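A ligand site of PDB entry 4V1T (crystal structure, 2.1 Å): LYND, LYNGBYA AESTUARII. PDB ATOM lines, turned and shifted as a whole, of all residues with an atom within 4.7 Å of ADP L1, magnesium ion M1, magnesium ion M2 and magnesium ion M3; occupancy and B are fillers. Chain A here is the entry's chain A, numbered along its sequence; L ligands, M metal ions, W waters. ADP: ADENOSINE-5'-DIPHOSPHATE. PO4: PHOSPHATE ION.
N of Glu 423 sits at hydrogen-bond distance from O4' of ADP L1, at 3.4 Å. An oxygen (O3') of ADP L1 lies within hydrogen-bond range of the backbone NH (N) of Ala 534 (2.9 Å). An oxygen (O2') of ADP L1 lies within hydrogen-bond range of the backbone carbonyl oxygen (O) of Ala 534 (2.4 Å). The side-chain carboxylate (OE1) of Glu 426 sits at hydrogen-bond distance from an oxygen (O3') of ADP L1, at 2.5 Å. NH1 of Arg 636 lies within salt-bridge range of O2A of ADP L1 (2.7 Å). The side-chain hydroxyl (OG) of Ser 419 sits at hydrogen-bond distance from an oxygen (O1A) of ADP L1, at 2.7 Å. The side-chain amino group (NZ) of Lys 409 sits close to an oxygen (O3B) of ADP L1. The side-chain amide nitrogen (NE2) of Gln 415 sits at hydrogen-bond distance from a nitrogen (N7) of ADP L1, at 3.1 Å. N1 of ADP L1 lies within hydrogen-bond range of ND2 of Asn 536 (3.1 Å). SG of Cys 422 lies within hydrogen-bond range of N3 of ADP L1, at 3.3 Å. NH1 of Arg 344 sits at hydrogen-bond distance from N3 of ADP L1, 3.3 Å away. NE2 of Gln 544 lies within hydrogen-bond range of O3A of ADP L1 (3.3 Å).
The side-chain amino group (NZ) of Lys 409 lies close to the side-chain carboxylate (OE2) of Glu 640 (3.3 Å). OE1 of Glu 640 sits at hydrogen-bond distance from N of Phe 624, 3.1 Å away. The guanidinium group (NH1) of Arg 427 lies within salt-bridge range of the side-chain carboxylate (OE2) of Glu 426, at 3.1 Å. The side-chain hydroxyl of Ser 419 lies within hydrogen-bond range of the backbone NH of Lys 409. The side-chain amide oxygen (OD1) of Asn 536 sits at hydrogen-bond distance from the side-chain hydroxyl (OG1) of Thr 351, at 2.6 Å. The side-chain carboxylate (OE2) of Glu 540 sits at hydrogen-bond distance from the side-chain amide nitrogen (ND2) of Asn 536 (2.7 Å). The side-chain sulfur of Cys 422 lies close to the backbone carbonyl oxygen of Ala 418 (3.2 Å). The side-chain amide oxygen (OE1) of Gln 544 lies within hydrogen-bond range of the guanidinium group (NH2) of Arg 344, at 2.7 Å.
Residues that only touch ADP L1: Ala 533 (3.4 Å), Thr 351 (3.9 Å), Glu 540 (3.9 Å) and Ala 418 (3.9 Å). Within 4 Å of ADP L1: Arg 344, Thr 351, Lys 409, Gln 415, Ala 418, Ser 419, Cys 422, Glu 423, Glu 426, Ala 533, Ala 534, Asn 536, Glu 540, Gln 544, Glu 548, Arg 636 and Glu 640. The nearest printed residue that does not touch ADP L1 is Gly 535 (4.0003 Å).
Merely in contact with magnesium ion M1: Arg 636 (3.97 Å) and Lys 409 (3.97 Å). Along chain A the residues within 4 Å of magnesium ion M1 span positions 409 to 640. The nearest printed residue that does not touch magnesium ion M1 is Glu 551 (4.02 Å).
Asn 532 touches magnesium ion M2 (O to MG, 3.9 Å). Two residues have an atom within 4 Å of magnesium ion M2: Asn 532 and Glu 548.
The nearest printed residue that does not touch magnesium ion M3 is Gln 643 (4.2 Å).
Magnesium ion M1 is bound by O3B of ADP L1 (2.0 Å). Magnesium ion M1 is bound by water W7, at 2.0 Å. O3 of PO4 L2 binds magnesium ion M1 (2.0 Å). Magnesium ion M1 is bound by OE2 of Glu 640, at 2.0 Å. Water W8 is bound to magnesium ion M1 (2.1 Å). Water W5 binds magnesium ion M1 (2.2 Å).
Magnesium ion M2 is bound by water W6 (1.9 Å), an oxygen (O2B) of ADP L1 (2.0 Å), an oxygen (O4) of PO4 L2 (2.0 Å), the side-chain carboxylate (OE2) of Glu 548 (2.0 Å), water W1 (2.1 Å) and water W10 (2.1 Å). Magnesium ion M2 has six donor atoms within binding distance.
Magnesium ion M3 is bound by O1 of PO4 L2, water W9, O1B of ADP L1, OE1 of Glu 423, water W3 and water W2.
Water W5 lies within hydrogen-bond range of OE1 of Glu 551 (2.7 Å), O of Phe 624 (2.7 Å), NH2 of Arg 636 (3.2 Å) and NZ of Lys 409 (3.5 Å). Water W8 lies within hydrogen-bond range of OE2 of Glu 551 and OE1 of Glu 640. Water W1 lies within hydrogen-bond range of the side-chain carboxylate of Glu 426 (2.7 Å) and the guanidinium group of Arg 427 (3.2 Å). Water W9 bridges OE2 of Glu 423 (2.6 Å) and NE2 of Gln 643 (3.4 Å). Water W3 lies within hydrogen-bond range of O1A of ADP L1, O of Ser 407 and NE2 of Gln 643. Water W4 lies within hydrogen-bond range of an oxygen (O2A) of ADP L1 (2.7 Å), the backbone carbonyl oxygen (O) of Lys 409 (2.8 Å) and the side-chain amide nitrogen (NE2) of Gln 415 (3.1 Å).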
ATOM      1  N   ARG A 344      18.184  -2.794  -6.825  1.00  0.00           N
ATOM      2  CA  ARG A 344      19.259  -2.009  -7.427  1.00  0.00           C
ATOM      3  C   ARG A 344      18.775  -0.605  -7.806  1.00  0.00           C
ATOM      4  O   ARG A 344      17.580  -0.341  -7.858  1.00  0.00           O
ATOM      5  CB  ARG A 344      19.829  -2.732  -8.643  1.00  0.00           C
ATOM      6  CG  ARG A 344      20.698  -3.932  -8.275  1.00  0.00           C
ATOM      7  CD  ARG A 344      21.181  -4.681  -9.492  1.00  0.00           C
ATOM      8  NE  ARG A 344      21.525  -6.074  -9.184  1.00  0.00           N
ATOM      9  CZ  ARG A 344      22.732  -6.515  -8.833  1.00  0.00           C
ATOM     10  NH1 ARG A 344      23.766  -5.686  -8.729  1.00  0.00           N
ATOM     11  NH2 ARG A 344      22.916  -7.800  -8.578  1.00  0.00           N
ATOM     12  N   PRO A 348      18.169  -2.899 -15.582  1.00  0.00           N
ATOM     13  CA  PRO A 348      19.155  -3.713 -16.300  1.00  0.00           C
ATOM     14  C   PRO A 348      19.342  -3.261 -17.745  1.00  0.00           C
ATOM     15  O   PRO A 348      20.432  -3.433 -18.294  1.00  0.00           O
ATOM     16  CB  PRO A 348      18.547  -5.124 -16.223  1.00  0.00           C
ATOM     17  CG  PRO A 348      17.077  -4.900 -16.054  1.00  0.00           C
ATOM     18  CD  PRO A 348      16.959  -3.658 -15.230  1.00  0.00           C
ATOM     19  N   THR A 351      21.967  -0.413 -17.433  1.00  0.00           N
ATOM     20  CA  THR A 351      23.304  -0.910 -17.130  1.00  0.00           C
ATOM     21  C   THR A 351      23.935  -1.519 -18.369  1.00  0.00           C
ATOM     22  O   THR A 351      25.126  -1.312 -18.652  1.00  0.00           O
ATOM     23  CB  THR A 351      23.283  -1.943 -15.989  1.00  0.00           C
ATOM     24  OG1 THR A 351      22.679  -1.377 -14.832  1.00  0.00           O
ATOM     25  CG2 THR A 351      24.720  -2.403 -15.651  1.00  0.00           C
ATOM     26  N   SER A 407      28.268 -16.380 -16.878  1.00  0.00           N
ATOM     27  CA  SER A 407      26.914 -16.697 -17.287  1.00  0.00           C
ATOM     28  C   SER A 407      25.944 -15.720 -16.646  1.00  0.00           C
ATOM     29  O   SER A 407      26.222 -15.155 -15.598  1.00  0.00           O
ATOM     30  CB  SER A 407      26.565 -18.144 -16.889  1.00  0.00           C
ATOM     31  OG  SER A 407      25.218 -18.439 -17.231  1.00  0.00           O
ATOM     32  N   LYS A 409      21.942 -14.876 -15.270  1.00  0.00           N
ATOM     33  CA  LYS A 409      20.892 -15.514 -14.495  1.00  0.00           C
ATOM     34  C   LYS A 409      19.734 -14.537 -14.433  1.00  0.00           C
ATOM     35  O   LYS A 409      19.947 -13.361 -14.141  1.00  0.00           O
ATOM     36  CB  LYS A 409      21.403 -15.757 -13.064  1.00  0.00           C
ATOM     37  CG  LYS A 409      21.077 -17.081 -12.458  1.00  0.00           C
ATOM     38  CD  LYS A 409      21.044 -16.984 -10.928  1.00  0.00           C
ATOM     39  CE  LYS A 409      22.255 -16.282 -10.334  1.00  0.00           C
ATOM     40  NZ  LYS A 409      22.102 -16.126  -8.859  1.00  0.00           N
ATOM     41  N   GLN A 415      17.256  -8.934 -17.216  1.00  0.00           N
ATOM     42  CA  GLN A 415      18.048  -9.129 -16.001  1.00  0.00           C
ATOM     43  C   GLN A 415      19.133 -10.182 -16.229  1.00  0.00           C
ATOM     44  O   GLN A 415      20.247 -10.061 -15.707  1.00  0.00           O
ATOM     45  CB  GLN A 415      17.142  -9.529 -14.842  1.00  0.00           C
ATOM     46  CG  GLN A 415      17.882  -9.996 -13.585  1.00  0.00           C
ATOM     47  CD  GLN A 415      19.021  -9.062 -13.183  1.00  0.00           C
ATOM     48  OE1 GLN A 415      18.974  -7.861 -13.410  1.00  0.00           O
ATOM     49  NE2 GLN A 415      20.072  -9.633 -12.596  1.00  0.00           N
ATOM     50  N   ALA A 418      21.997  -8.465 -18.097  1.00  0.00           N
ATOM     51  CA  ALA A 418      22.800  -7.634 -17.240  1.00  0.00           C
ATOM     52  C   ALA A 418      23.663  -8.486 -16.315  1.00  0.00           C
ATOM     53  O   ALA A 418      24.813  -8.170 -16.071  1.00  0.00           O
ATOM     54  CB  ALA A 418      21.899  -6.716 -16.433  1.00  0.00           C
ATOM     55  N   SER A 419      23.077  -9.560 -15.811  1.00  0.00           N
ATOM     56  CA  SER A 419      23.769 -10.516 -14.951  1.00  0.00           C
ATOM     57  C   SER A 419      24.998 -11.067 -15.664  1.00  0.00           C
ATOM     58  O   SER A 419      26.085 -11.097 -15.110  1.00  0.00           O
ATOM     59  CB  SER A 419      22.833 -11.656 -14.547  1.00  0.00           C
ATOM     60  OG  SER A 419      23.531 -12.720 -13.909  1.00  0.00           O
ATOM     61  N   CYS A 422      27.620  -8.196 -16.399  1.00  0.00           N
ATOM     62  CA  CYS A 422      28.252  -7.682 -15.196  1.00  0.00           C
ATOM     63  C   CYS A 422      29.153  -8.720 -14.514  1.00  0.00           C
ATOM     64  O   CYS A 422      30.165  -8.367 -13.925  1.00  0.00           O
ATOM     65  CB  CYS A 422      27.188  -7.164 -14.238  1.00  0.00           C
ATOM     66  SG  CYS A 422      26.381  -5.655 -14.822  1.00  0.00           S
ATOM     67  N   GLU A 423      28.790  -9.995 -14.600  1.00  0.00           N
ATOM     68  CA  GLU A 423      29.666 -11.045 -14.083  1.00  0.00           C
ATOM     69  C   GLU A 423      30.953 -11.087 -14.877  1.00  0.00           C
ATOM     70  O   GLU A 423      32.027 -11.196 -14.302  1.00  0.00           O
ATOM     71  CB  GLU A 423      28.983 -12.424 -14.105  1.00  0.00           C
ATOM     72  CG  GLU A 423      29.865 -13.513 -13.477  1.00  0.00           C
ATOM     73  CD  GLU A 423      29.153 -14.820 -13.258  1.00  0.00           C
ATOM     74  OE1 GLU A 423      28.419 -14.940 -12.264  1.00  0.00           O
ATOM     75  OE2 GLU A 423      29.307 -15.736 -14.093  1.00  0.00           O
ATOM     76  N   GLU A 426      32.905  -8.343 -13.759  1.00  0.00           N
ATOM     77  CA  GLU A 426      33.292  -8.676 -12.384  1.00  0.00           C
ATOM     78  C   GLU A 426      34.570  -9.521 -12.378  1.00  0.00           C
ATOM     79  O   GLU A 426      35.513  -9.192 -11.667  1.00  0.00           O
ATOM     80  CB  GLU A 426      32.152  -9.412 -11.678  1.00  0.00           C
ATOM     81  CG  GLU A 426      32.476  -9.930 -10.286  1.00  0.00           C
ATOM     82  CD  GLU A 426      31.619 -11.136  -9.893  1.00  0.00           C
ATOM     83  OE1 GLU A 426      30.377 -11.075 -10.028  1.00  0.00           O
ATOM     84  OE2 GLU A 426      32.200 -12.152  -9.430  1.00  0.00           O
ATOM     85  N   ARG A 427      34.594 -10.594 -13.168  1.00  0.00           N
ATOM     86  CA  ARG A 427      35.737 -11.511 -13.187  1.00  0.00           C
ATOM     87  C   ARG A 427      37.006 -10.838 -13.712  1.00  0.00           C
ATOM     88  O   ARG A 427      38.077 -11.044 -13.169  1.00  0.00           O
ATOM     89  CB  ARG A 427      35.485 -12.763 -14.035  1.00  0.00           C
ATOM     90  CG  ARG A 427      34.135 -13.436 -13.883  1.00  0.00           C
ATOM     91  CD  ARG A 427      33.643 -13.608 -12.458  1.00  0.00           C
ATOM     92  NE  ARG A 427      33.975 -14.917 -11.908  1.00  0.00           N
ATOM     93  CZ  ARG A 427      33.256 -15.569 -11.003  1.00  0.00           C
ATOM     94  NH1 ARG A 427      32.133 -15.050 -10.512  1.00  0.00           N
ATOM     95  NH2 ARG A 427      33.670 -16.762 -10.571  1.00  0.00           N
ATOM     96  N   ASN A 532      32.980 -11.718  -4.235  1.00  0.00           N
ATOM     97  CA  ASN A 532      33.207 -10.806  -5.365  1.00  0.00           C
ATOM     98  C   ASN A 532      31.878 -10.433  -6.024  1.00  0.00           C
ATOM     99  O   ASN A 532      31.033 -11.284  -6.255  1.00  0.00           O
ATOM    100  CB  ASN A 532      34.140 -11.419  -6.407  1.00  0.00           C
ATOM    101  CG  ASN A 532      35.514 -11.762  -5.849  1.00  0.00           C
ATOM    102  OD1 ASN A 532      35.640 -12.413  -4.810  1.00  0.00           O
ATOM    103  ND2 ASN A 532      36.561 -11.336  -6.557  1.00  0.00           N
ATOM    104  N   ALA A 533      31.699  -9.157  -6.337  1.00  0.00           N
ATOM    105  CA  ALA A 533      30.459  -8.711  -6.978  1.00  0.00           C
ATOM    106  C   ALA A 533      30.587  -7.385  -7.696  1.00  0.00           C
ATOM    107  O   ALA A 533      31.298  -6.486  -7.250  1.00  0.00           O
ATOM    108  CB  ALA A 533      29.356  -8.625  -5.944  1.00  0.00           C
ATOM    109  N   ALA A 534      29.881  -7.266  -8.808  1.00  0.00           N
ATOM    110  CA  ALA A 534      29.776  -6.003  -9.545  1.00  0.00           C
ATOM    111  C   ALA A 534      28.470  -5.286  -9.226  1.00  0.00           C
ATOM    112  O   ALA A 534      27.532  -5.893  -8.749  1.00  0.00           O
ATOM    113  CB  ALA A 534      29.897  -6.255 -11.037  1.00  0.00           C
ATOM    114  N   GLY A 535      28.436  -3.989  -9.498  1.00  0.00           N
ATOM    115  CA  GLY A 535      27.230  -3.205  -9.252  1.00  0.00           C
ATOM    116  C   GLY A 535      27.319  -1.849  -9.897  1.00  0.00           C
ATOM    117  O   GLY A 535      28.400  -1.405 -10.264  1.00  0.00           O
ATOM    118  N   ASN A 536      26.174  -1.182 -10.019  1.00  0.00           N
ATOM    119  CA  ASN A 536      26.124   0.159 -10.615  1.00  0.00           C
ATOM    120  C   ASN A 536      26.737   1.217  -9.703  1.00  0.00           C
ATOM    121  O   ASN A 536      27.053   2.314 -10.148  1.00  0.00           O
ATOM    122  CB  ASN A 536      24.685   0.534 -10.961  1.00  0.00           C
ATOM    123  CG  ASN A 536      24.057  -0.425 -11.950  1.00  0.00           C
ATOM    124  OD1 ASN A 536      24.318  -0.366 -13.153  1.00  0.00           O
ATOM    125  ND2 ASN A 536      23.221  -1.314 -11.446  1.00  0.00           N
ATOM    126  N   GLU A 540      26.056  -0.922  -3.886  1.00  0.00           N
ATOM    127  CA  GLU A 540      25.274  -1.962  -4.561  1.00  0.00           C
ATOM    128  C   GLU A 540      26.106  -3.240  -4.662  1.00  0.00           C
ATOM    129  O   GLU A 540      25.637  -4.339  -4.383  1.00  0.00           O
ATOM    130  CB  GLU A 540      24.879  -1.485  -5.956  1.00  0.00           C
ATOM    131  CG  GLU A 540      23.636  -2.124  -6.532  1.00  0.00           C
ATOM    132  CD  GLU A 540      23.284  -1.558  -7.890  1.00  0.00           C
ATOM    133  OE1 GLU A 540      22.729  -0.437  -7.950  1.00  0.00           O
ATOM    134  OE2 GLU A 540      23.575  -2.227  -8.906  1.00  0.00           O
ATOM    135  N   GLN A 544      25.727  -7.013  -2.564  1.00  0.00           N
ATOM    136  CA  GLN A 544      25.661  -8.283  -3.261  1.00  0.00           C
ATOM    137  C   GLN A 544      26.793  -9.214  -2.813  1.00  0.00           C
ATOM    138  O   GLN A 544      26.580 -10.414  -2.596  1.00  0.00           O
ATOM    139  CB  GLN A 544      25.725  -8.085  -4.773  1.00  0.00           C
ATOM    140  CG  GLN A 544      25.934  -9.384  -5.549  1.00  0.00           C
ATOM    141  CD  GLN A 544      24.733  -9.804  -6.359  1.00  0.00           C
ATOM    142  OE1 GLN A 544      23.687  -9.159  -6.341  1.00  0.00           O
ATOM    143  NE2 GLN A 544      24.890 -10.914  -7.097  1.00  0.00           N
ATOM    144  N   GLU A 548      26.447 -12.883  -1.014  1.00  0.00           N
ATOM    145  CA  GLU A 548      27.078 -14.072  -1.564  1.00  0.00           C
ATOM    146  C   GLU A 548      27.820 -14.839  -0.449  1.00  0.00           C
ATOM    147  O   GLU A 548      27.812 -16.063  -0.421  1.00  0.00           O
ATOM    148  CB  GLU A 548      28.047 -13.719  -2.696  1.00  0.00           C
ATOM    149  CG  GLU A 548      28.571 -14.944  -3.444  1.00  0.00           C
ATOM    150  CD  GLU A 548      29.335 -14.588  -4.705  1.00  0.00           C
ATOM    151  OE1 GLU A 548      30.563 -14.304  -4.604  1.00  0.00           O
ATOM    152  OE2 GLU A 548      28.707 -14.587  -5.795  1.00  0.00           O
ATOM    153  N   GLU A 551      25.269 -16.620   1.643  1.00  0.00           N
ATOM    154  CA  GLU A 551      24.818 -17.741   0.825  1.00  0.00           C
ATOM    155  C   GLU A 551      25.742 -18.939   0.988  1.00  0.00           C
ATOM    156  O   GLU A 551      25.309 -20.026   1.354  1.00  0.00           O
ATOM    157  CB  GLU A 551      24.726 -17.322  -0.644  1.00  0.00           C
ATOM    158  CG  GLU A 551      24.440 -18.439  -1.640  1.00  0.00           C
ATOM    159  CD  GLU A 551      24.982 -18.136  -3.033  1.00  0.00           C
ATOM    160  OE1 GLU A 551      24.802 -17.002  -3.515  1.00  0.00           O
ATOM    161  OE2 GLU A 551      25.580 -19.027  -3.658  1.00  0.00           O
ATOM    162  N   ARG A 552      27.026 -18.737   0.720  1.00  0.00           N
ATOM    163  CA  ARG A 552      27.997 -19.824   0.753  1.00  0.00           C
ATOM    164  C   ARG A 552      28.154 -20.382   2.160  1.00  0.00           C
ATOM    165  O   ARG A 552      28.322 -21.581   2.337  1.00  0.00           O
ATOM    166  CB  ARG A 552      29.371 -19.360   0.237  1.00  0.00           C
ATOM    167  CG  ARG A 552      29.349 -18.745  -1.146  1.00  0.00           C
ATOM    168  CD  ARG A 552      28.819 -19.673  -2.199  1.00  0.00           C
ATOM    169  NE  ARG A 552      28.644 -19.012  -3.490  1.00  0.00           N
ATOM    170  CZ  ARG A 552      29.660 -18.594  -4.255  1.00  0.00           C
ATOM    171  NH1 ARG A 552      30.916 -18.707  -3.846  1.00  0.00           N
ATOM    172  NH2 ARG A 552      29.414 -18.055  -5.433  1.00  0.00           N
ATOM    173  N   PHE A 624      21.785 -21.577  -5.425  1.00  0.00           N
ATOM    174  CA  PHE A 624      21.712 -20.903  -4.137  1.00  0.00           C
ATOM    175  C   PHE A 624      21.495 -19.401  -4.265  1.00  0.00           C
ATOM    176  O   PHE A 624      21.801 -18.805  -5.289  1.00  0.00           O
ATOM    177  CB  PHE A 624      22.987 -21.173  -3.337  1.00  0.00           C
ATOM    178  CG  PHE A 624      23.469 -22.613  -3.424  1.00  0.00           C
ATOM    179  CD1 PHE A 624      22.770 -23.629  -2.811  1.00  0.00           C
ATOM    180  CD2 PHE A 624      24.623 -22.922  -4.122  1.00  0.00           C
ATOM    181  CE1 PHE A 624      23.208 -24.940  -2.894  1.00  0.00           C
ATOM    182  CE2 PHE A 624      25.067 -24.225  -4.225  1.00  0.00           C
ATOM    183  CZ  PHE A 624      24.357 -25.234  -3.607  1.00  0.00           C
ATOM    184  N   ARG A 636      16.859 -15.905  -6.741  1.00  0.00           N
ATOM    185  CA  ARG A 636      18.240 -16.123  -7.106  1.00  0.00           C
ATOM    186  C   ARG A 636      18.577 -17.600  -7.125  1.00  0.00           C
ATOM    187  O   ARG A 636      19.256 -18.077  -8.029  1.00  0.00           O
ATOM    188  CB  ARG A 636      19.169 -15.384  -6.132  1.00  0.00           C
ATOM    189  CG  ARG A 636      19.176 -13.869  -6.311  1.00  0.00           C
ATOM    190  CD  ARG A 636      20.194 -13.228  -5.379  1.00  0.00           C
ATOM    191  NE  ARG A 636      21.534 -13.800  -5.579  1.00  0.00           N
ATOM    192  CZ  ARG A 636      22.304 -13.568  -6.650  1.00  0.00           C
ATOM    193  NH1 ARG A 636      21.872 -12.759  -7.620  1.00  0.00           N
ATOM    194  NH2 ARG A 636      23.495 -14.139  -6.745  1.00  0.00           N
ATOM    195  N   GLU A 640      19.341 -19.847 -10.556  1.00  0.00           N
ATOM    196  CA  GLU A 640      20.658 -20.463 -10.664  1.00  0.00           C
ATOM    197  C   GLU A 640      20.528 -21.947 -11.019  1.00  0.00           C
ATOM    198  O   GLU A 640      21.364 -22.496 -11.722  1.00  0.00           O
ATOM    199  CB  GLU A 640      21.472 -20.295  -9.384  1.00  0.00           C
ATOM    200  CG  GLU A 640      22.971 -20.258  -9.612  1.00  0.00           C
ATOM    201  CD  GLU A 640      23.746 -19.829  -8.390  1.00  0.00           C
ATOM    202  OE1 GLU A 640      23.911 -20.654  -7.483  1.00  0.00           O
ATOM    203  OE2 GLU A 640      24.216 -18.652  -8.347  1.00  0.00           O
ATOM    204  N   GLN A 643      20.165 -21.909 -14.565  1.00  0.00           N
ATOM    205  CA  GLN A 643      21.430 -21.554 -15.175  1.00  0.00           C
ATOM    206  C   GLN A 643      22.337 -22.774 -15.391  1.00  0.00           C
ATOM    207  O   GLN A 643      22.923 -22.950 -16.448  1.00  0.00           O
ATOM    208  CB  GLN A 643      22.151 -20.546 -14.290  1.00  0.00           C
ATOM    209  CG  GLN A 643      23.394 -19.922 -14.884  1.00  0.00           C
ATOM    210  CD  GLN A 643      23.984 -18.872 -13.951  1.00  0.00           C
ATOM    211  OE1 GLN A 643      23.923 -19.001 -12.737  1.00  0.00           O
ATOM    212  NE2 GLN A 643      24.534 -17.819 -14.531  1.00  0.00           N
HETATM  213  PB  ADP L   1      25.912 -14.772  -9.041  1.00  0.00           P
HETATM  214  O1B ADP L   1      26.510 -14.970 -10.407  1.00  0.00           O
HETATM  215  O2B ADP L   1      26.880 -14.319  -7.975  1.00  0.00           O
HETATM  216  O3B ADP L   1      25.056 -15.931  -8.607  1.00  0.00           O
HETATM  217  PA  ADP L   1      24.154 -12.935 -10.452  1.00  0.00           P
HETATM  218  O1A ADP L   1      24.147 -13.921 -11.562  1.00  0.00           O
HETATM  219  O2A ADP L   1      22.846 -12.359 -10.060  1.00  0.00           O
HETATM  220  O3A ADP L   1      24.874 -13.521  -9.132  1.00  0.00           O
HETATM  221  O5' ADP L   1      25.057 -11.699 -10.884  1.00  0.00           O
HETATM  222  C5' ADP L   1      26.303 -11.850 -11.557  1.00  0.00           C
HETATM  223  C4' ADP L   1      27.119 -10.569 -11.352  1.00  0.00           C
HETATM  224  O4' ADP L   1      26.552  -9.484 -12.104  1.00  0.00           O
HETATM  225  C3' ADP L   1      27.134 -10.139  -9.899  1.00  0.00           C
HETATM  226  O3' ADP L   1      28.416  -9.619  -9.597  1.00  0.00           O
HETATM  227  C2' ADP L   1      26.095  -9.033  -9.807  1.00  0.00           C
HETATM  228  O2' ADP L   1      26.406  -8.050  -8.828  1.00  0.00           O
HETATM  229  C1' ADP L   1      26.112  -8.460 -11.202  1.00  0.00           C
HETATM  230  N9  ADP L   1      24.762  -7.984 -11.589  1.00  0.00           N
HETATM  231  C8  ADP L   1      23.682  -8.752 -11.806  1.00  0.00           C
HETATM  232  N7  ADP L   1      22.628  -7.979 -12.174  1.00  0.00           N
HETATM  233  C5  ADP L   1      23.048  -6.690 -12.181  1.00  0.00           C
HETATM  234  C6  ADP L   1      22.448  -5.376 -12.477  1.00  0.00           C
HETATM  235  N6  ADP L   1      21.152  -5.258 -12.840  1.00  0.00           N
HETATM  236  N1  ADP L   1      23.257  -4.300 -12.365  1.00  0.00           N
HETATM  237  C2  ADP L   1      24.537  -4.381 -12.011  1.00  0.00           C
HETATM  238  N3  ADP L   1      25.140  -5.552 -11.727  1.00  0.00           N
HETATM  239  C4  ADP L   1      24.468  -6.707 -11.798  1.00  0.00           C
HETATM  240  P   PO4 L   2      28.630 -17.356  -8.931  1.00  0.00           P
HETATM  241  O1  PO4 L   2      28.528 -17.140 -10.423  1.00  0.00           O
HETATM  242  O2  PO4 L   2      29.722 -18.402  -8.679  1.00  0.00           O
HETATM  243  O3  PO4 L   2      27.297 -17.844  -8.389  1.00  0.00           O
HETATM  244  O4  PO4 L   2      29.003 -16.071  -8.241  1.00  0.00           O
HETATM  245 MG    MG M   1      25.565 -17.457  -7.439  1.00  0.00          MG
HETATM  246 MG    MG M   2      28.864 -14.100  -7.770  1.00  0.00          MG
HETATM  247 MG    MG M   3      27.222 -16.465 -11.605  1.00  0.00          MG
HETATM  248  O   HOH W   1      29.350 -13.606  -9.773  1.00  0.00           O
HETATM  249  O   HOH W   2      25.170 -17.447 -10.816  1.00  0.00           O
HETATM  250  O   HOH W   3      25.797 -15.498 -12.848  1.00  0.00           O
HETATM  251  O   HOH W   4      20.630 -12.541 -11.554  1.00  0.00           O
HETATM  252  O   HOH W   5      23.904 -17.229  -6.074  1.00  0.00           O
HETATM  253  O   HOH W   6      30.734 -14.073  -7.536  1.00  0.00           O
HETATM  254  O   HOH W   7      26.433 -16.489  -5.907  1.00  0.00           O
HETATM  255  O   HOH W   8      25.843 -19.072  -6.146  1.00  0.00           O
HETATM  256  O   HOH W   9      27.700 -17.618 -13.219  1.00  0.00           O
HETATM  257  O   HOH W  10      28.603 -12.086  -7.113  1.00  0.00           O
